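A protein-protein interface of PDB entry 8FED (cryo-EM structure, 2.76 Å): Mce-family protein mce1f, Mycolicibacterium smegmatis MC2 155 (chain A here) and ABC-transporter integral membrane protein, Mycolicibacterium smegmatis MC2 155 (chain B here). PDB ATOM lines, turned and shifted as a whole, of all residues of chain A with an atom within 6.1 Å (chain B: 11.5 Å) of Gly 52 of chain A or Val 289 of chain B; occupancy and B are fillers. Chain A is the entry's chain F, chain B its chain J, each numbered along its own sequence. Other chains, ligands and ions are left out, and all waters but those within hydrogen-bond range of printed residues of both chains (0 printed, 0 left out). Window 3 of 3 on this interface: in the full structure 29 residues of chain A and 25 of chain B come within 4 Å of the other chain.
Along chain B the printed residues that touch a printed residue of chain A span positions 286 to 289. Among the printed residues, 5 pairs touch across the chains. Among the printed residues, no Asp or Glu carboxylate lies within 4 Å of a Lys or Arg side-chain nitrogen of the other chain.
Gly 52 of chain A touches Val 289 of chain B (CA to CG1, 3.6 Å). CG of Tyr 54 of chain A touches CB of Asn 286 of chain B, 3.5 Å away. CA of Gly 106 of chain A touches O of Leu 287 of chain B, at 3.4 Å. Leu 287 of chain B touches Gln 108 of chain A. Val 289 of chain B touches Gln 108 of chain A.
Gly 52 of chain A touches just one residue of chain B: Val 289 (3.6 Å). Val 289 of chain B touches two residues of chain A. No residue of chain B comes within 4 Å of Ser 50 of chain A. No residue of chain B comes within 4 Å of Gly 51 of chain A. No residue of chain B comes within 4 Å of Leu 53 of chain A. Printed residues of chain B within 4 Å of Gly 106 of chain A: Leu 287. Printed residues of chain B within 4 Å of Gln 108 of chain A: Leu 287 and Val 289. Printed residues of chain A within 4 Å of Leu 287 of chain B: Gly 106 and Gln 108. Printed residues of chain A within 4 Å of Asn 286 of chain B: Tyr 54. The nearest residue of chain A that does not touch Val 289 of chain B is Gly 51 of chain A (4.1 Å).
OE1 of Gln 108 of chain A lies close to O of Gly 51 of chain A (3.0 Å). The backbone carbonyl oxygen of Gln 108 of chain A is in hydrogen-bond range of the side-chain hydroxyl of Tyr 54 of chain A.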
ATOM      1  N   ASN A  49      -7.900 -16.564  -4.564  1.00  0.00           N
ATOM      2  CA  ASN A  49      -8.046 -16.012  -3.228  1.00  0.00           C
ATOM      3  C   ASN A  49      -7.267 -14.708  -3.200  1.00  0.00           C
ATOM      4  O   ASN A  49      -6.325 -14.523  -3.974  1.00  0.00           O
ATOM      5  CB  ASN A  49      -7.536 -16.983  -2.156  1.00  0.00           C
ATOM      6  CG  ASN A  49      -7.948 -16.579  -0.757  1.00  0.00           C
ATOM      7  OD1 ASN A  49      -7.312 -15.736  -0.127  1.00  0.00           O
ATOM      8  ND2 ASN A  49      -9.016 -17.188  -0.258  1.00  0.00           N
ATOM      9  N   SER A  50      -7.667 -13.801  -2.310  1.00  0.00           N
ATOM     10  CA  SER A  50      -6.995 -12.509  -2.238  1.00  0.00           C
ATOM     11  C   SER A  50      -5.544 -12.650  -1.807  1.00  0.00           C
ATOM     12  O   SER A  50      -4.673 -11.909  -2.277  1.00  0.00           O
ATOM     13  CB  SER A  50      -7.733 -11.587  -1.278  1.00  0.00           C
ATOM     14  OG  SER A  50      -7.039 -10.364  -1.116  1.00  0.00           O
ATOM     15  N   GLY A  51      -5.261 -13.595  -0.915  1.00  0.00           N
ATOM     16  CA  GLY A  51      -3.910 -13.736  -0.420  1.00  0.00           C
ATOM     17  C   GLY A  51      -3.490 -12.619   0.500  1.00  0.00           C
ATOM     18  O   GLY A  51      -2.293 -12.364   0.650  1.00  0.00           O
ATOM     19  N   GLY A  52      -4.450 -11.942   1.128  1.00  0.00           N
ATOM     20  CA  GLY A  52      -4.166 -10.808   1.975  1.00  0.00           C
ATOM     21  C   GLY A  52      -3.980  -9.488   1.264  1.00  0.00           C
ATOM     22  O   GLY A  52      -3.653  -8.495   1.923  1.00  0.00           O
ATOM     23  N   LEU A  53      -4.170  -9.442  -0.052  1.00  0.00           N
ATOM     24  CA  LEU A  53      -3.991  -8.201  -0.790  1.00  0.00           C
ATOM     25  C   LEU A  53      -5.048  -7.182  -0.381  1.00  0.00           C
ATOM     26  O   LEU A  53      -6.195  -7.531  -0.096  1.00  0.00           O
ATOM     27  CB  LEU A  53      -4.066  -8.465  -2.293  1.00  0.00           C
ATOM     28  CG  LEU A  53      -3.524  -7.379  -3.217  1.00  0.00           C
ATOM     29  CD1 LEU A  53      -2.073  -7.096  -2.897  1.00  0.00           C
ATOM     30  CD2 LEU A  53      -3.674  -7.796  -4.665  1.00  0.00           C
ATOM     31  N   TYR A  54      -4.644  -5.914  -0.348  1.00  0.00           N
ATOM     32  CA  TYR A  54      -5.499  -4.827   0.100  1.00  0.00           C
ATOM     33  C   TYR A  54      -5.344  -3.647  -0.847  1.00  0.00           C
ATOM     34  O   TYR A  54      -4.416  -3.592  -1.657  1.00  0.00           O
ATOM     35  CB  TYR A  54      -5.168  -4.417   1.541  1.00  0.00           C
ATOM     36  CG  TYR A  54      -3.687  -4.239   1.810  1.00  0.00           C
ATOM     37  CD1 TYR A  54      -3.037  -3.059   1.480  1.00  0.00           C
ATOM     38  CD2 TYR A  54      -2.943  -5.249   2.401  1.00  0.00           C
ATOM     39  CE1 TYR A  54      -1.693  -2.891   1.723  1.00  0.00           C
ATOM     40  CE2 TYR A  54      -1.595  -5.090   2.649  1.00  0.00           C
ATOM     41  CZ  TYR A  54      -0.975  -3.908   2.308  1.00  0.00           C
ATOM     42  OH  TYR A  54       0.367  -3.739   2.550  1.00  0.00           O
ATOM     43  N   VAL A  99       0.283 -12.912  -5.733  1.00  0.00           N
ATOM     44  CA  VAL A  99       0.226 -12.185  -4.473  1.00  0.00           C
ATOM     45  C   VAL A  99       1.385 -12.635  -3.596  1.00  0.00           C
ATOM     46  O   VAL A  99       1.719 -13.825  -3.541  1.00  0.00           O
ATOM     47  CB  VAL A  99      -1.129 -12.408  -3.785  1.00  0.00           C
ATOM     48  CG1 VAL A  99      -1.228 -11.585  -2.514  1.00  0.00           C
ATOM     49  CG2 VAL A  99      -2.260 -12.059  -4.734  1.00  0.00           C
ATOM     50  N   GLY A 106       4.037  -8.769   7.425  1.00  0.00           N
ATOM     51  CA  GLY A 106       2.967  -8.356   6.539  1.00  0.00           C
ATOM     52  C   GLY A 106       3.450  -7.692   5.268  1.00  0.00           C
ATOM     53  O   GLY A 106       4.348  -8.207   4.597  1.00  0.00           O
ATOM     54  N   GLN A 108       1.623  -6.942   2.282  1.00  0.00           N
ATOM     55  CA  GLN A 108       1.188  -7.678   1.104  1.00  0.00           C
ATOM     56  C   GLN A 108       1.296  -6.811  -0.146  1.00  0.00           C
ATOM     57  O   GLN A 108       1.145  -5.589  -0.099  1.00  0.00           O
ATOM     58  CB  GLN A 108      -0.250  -8.158   1.279  1.00  0.00           C
ATOM     59  CG  GLN A 108      -0.486  -8.926   2.563  1.00  0.00           C
ATOM     60  CD  GLN A 108       0.194 -10.274   2.564  1.00  0.00           C
ATOM     61  OE1 GLN A 108       0.235 -10.962   1.545  1.00  0.00           O
ATOM     62  NE2 GLN A 108       0.745 -10.657   3.709  1.00  0.00           N
ATOM     63  N   PHE B 214       2.565   3.700   2.955  1.00  0.00           N
ATOM     64  CA  PHE B 214       1.591   3.689   4.039  1.00  0.00           C
ATOM     65  C   PHE B 214       0.935   5.044   4.271  1.00  0.00           C
ATOM     66  O   PHE B 214       0.213   5.209   5.258  1.00  0.00           O
ATOM     67  CB  PHE B 214       2.253   3.197   5.328  1.00  0.00           C
ATOM     68  CG  PHE B 214       2.734   1.777   5.254  1.00  0.00           C
ATOM     69  CD1 PHE B 214       1.893   0.731   5.591  1.00  0.00           C
ATOM     70  CD2 PHE B 214       4.022   1.486   4.843  1.00  0.00           C
ATOM     71  CE1 PHE B 214       2.328  -0.575   5.521  1.00  0.00           C
ATOM     72  CE2 PHE B 214       4.462   0.180   4.770  1.00  0.00           C
ATOM     73  CZ  PHE B 214       3.614  -0.850   5.111  1.00  0.00           C
ATOM     74  N   ARG B 216      -1.783   7.765   2.941  1.00  0.00           N
ATOM     75  CA  ARG B 216      -2.945   7.943   2.082  1.00  0.00           C
ATOM     76  C   ARG B 216      -3.260   9.427   1.972  1.00  0.00           C
ATOM     77  O   ARG B 216      -3.260  10.143   2.978  1.00  0.00           O
ATOM     78  CB  ARG B 216      -4.154   7.177   2.624  1.00  0.00           C
ATOM     79  CG  ARG B 216      -4.090   5.672   2.409  1.00  0.00           C
ATOM     80  CD  ARG B 216      -3.574   4.953   3.643  1.00  0.00           C
ATOM     81  NE  ARG B 216      -3.421   3.519   3.424  1.00  0.00           N
ATOM     82  CZ  ARG B 216      -4.407   2.636   3.511  1.00  0.00           C
ATOM     83  NH1 ARG B 216      -5.646   3.007   3.789  1.00  0.00           N
ATOM     84  NH2 ARG B 216      -4.144   1.348   3.314  1.00  0.00           N
ATOM     85  N   PRO B 283     -10.036   2.013  10.307  1.00  0.00           N
ATOM     86  CA  PRO B 283      -8.750   2.637  10.656  1.00  0.00           C
ATOM     87  C   PRO B 283      -7.986   3.190   9.467  1.00  0.00           C
ATOM     88  O   PRO B 283      -7.071   3.998   9.675  1.00  0.00           O
ATOM     89  CB  PRO B 283      -7.978   1.494  11.327  1.00  0.00           C
ATOM     90  CG  PRO B 283      -8.587   0.259  10.768  1.00  0.00           C
ATOM     91  CD  PRO B 283     -10.040   0.566  10.574  1.00  0.00           C
ATOM     92  N   PHE B 285      -5.835   1.648   7.355  1.00  0.00           N
ATOM     93  CA  PHE B 285      -4.451   1.199   7.452  1.00  0.00           C
ATOM     94  C   PHE B 285      -4.421  -0.321   7.391  1.00  0.00           C
ATOM     95  O   PHE B 285      -5.098  -0.985   8.180  1.00  0.00           O
ATOM     96  CB  PHE B 285      -3.798   1.702   8.744  1.00  0.00           C
ATOM     97  CG  PHE B 285      -2.486   1.052   9.047  1.00  0.00           C
ATOM     98  CD1 PHE B 285      -1.375   1.317   8.270  1.00  0.00           C
ATOM     99  CD2 PHE B 285      -2.359   0.188  10.117  1.00  0.00           C
ATOM    100  CE1 PHE B 285      -0.170   0.717   8.547  1.00  0.00           C
ATOM    101  CE2 PHE B 285      -1.153  -0.413  10.401  1.00  0.00           C
ATOM    102  CZ  PHE B 285      -0.058  -0.148   9.615  1.00  0.00           C
ATOM    103  N   ASN B 286      -3.637  -0.864   6.458  1.00  0.00           N
ATOM    104  CA  ASN B 286      -3.517  -2.304   6.268  1.00  0.00           C
ATOM    105  C   ASN B 286      -2.048  -2.694   6.220  1.00  0.00           C
ATOM    106  O   ASN B 286      -1.280  -2.136   5.431  1.00  0.00           O
ATOM    107  CB  ASN B 286      -4.213  -2.753   4.978  1.00  0.00           C
ATOM    108  CG  ASN B 286      -5.703  -2.487   4.994  1.00  0.00           C
ATOM    109  OD1 ASN B 286      -6.151  -1.386   4.679  1.00  0.00           O
ATOM    110  ND2 ASN B 286      -6.480  -3.499   5.355  1.00  0.00           N
ATOM    111  N   LEU B 287      -1.657  -3.635   7.077  1.00  0.00           N
ATOM    112  CA  LEU B 287      -0.344  -4.266   7.006  1.00  0.00           C
ATOM    113  C   LEU B 287      -0.426  -5.776   6.843  1.00  0.00           C
ATOM    114  O   LEU B 287       0.273  -6.342   5.995  1.00  0.00           O
ATOM    115  CB  LEU B 287       0.486  -3.925   8.253  1.00  0.00           C
ATOM    116  CG  LEU B 287       1.911  -4.479   8.233  1.00  0.00           C
ATOM    117  CD1 LEU B 287       2.716  -3.844   7.112  1.00  0.00           C
ATOM    118  CD2 LEU B 287       2.594  -4.265   9.566  1.00  0.00           C
ATOM    119  N   THR B 288      -1.260  -6.447   7.633  1.00  0.00           N
ATOM    120  CA  THR B 288      -1.353  -7.899   7.618  1.00  0.00           C
ATOM    121  C   THR B 288      -2.435  -8.339   6.631  1.00  0.00           C
ATOM    122  O   THR B 288      -2.953  -7.542   5.845  1.00  0.00           O
ATOM    123  CB  THR B 288      -1.620  -8.424   9.026  1.00  0.00           C
ATOM    124  OG1 THR B 288      -1.705  -9.854   8.998  1.00  0.00           O
ATOM    125  CG2 THR B 288      -2.920  -7.855   9.571  1.00  0.00           C
ATOM    126  N   VAL B 289      -2.792  -9.620   6.666  1.00  0.00           N
ATOM    127  CA  VAL B 289      -3.774 -10.156   5.733  1.00  0.00           C
ATOM    128  C   VAL B 289      -5.182  -9.963   6.285  1.00  0.00           C
ATOM    129  O   VAL B 289      -6.171 -10.152   5.578  1.00  0.00           O
ATOM    130  CB  VAL B 289      -3.516 -11.648   5.439  1.00  0.00           C
ATOM    131  CG1 VAL B 289      -2.174 -11.841   4.748  1.00  0.00           C
ATOM    132  CG2 VAL B 289      -3.610 -12.471   6.694  1.00  0.00           C
ATOM    133  OXT VAL B 289      -5.367  -9.619   7.452  1.00  0.00           O
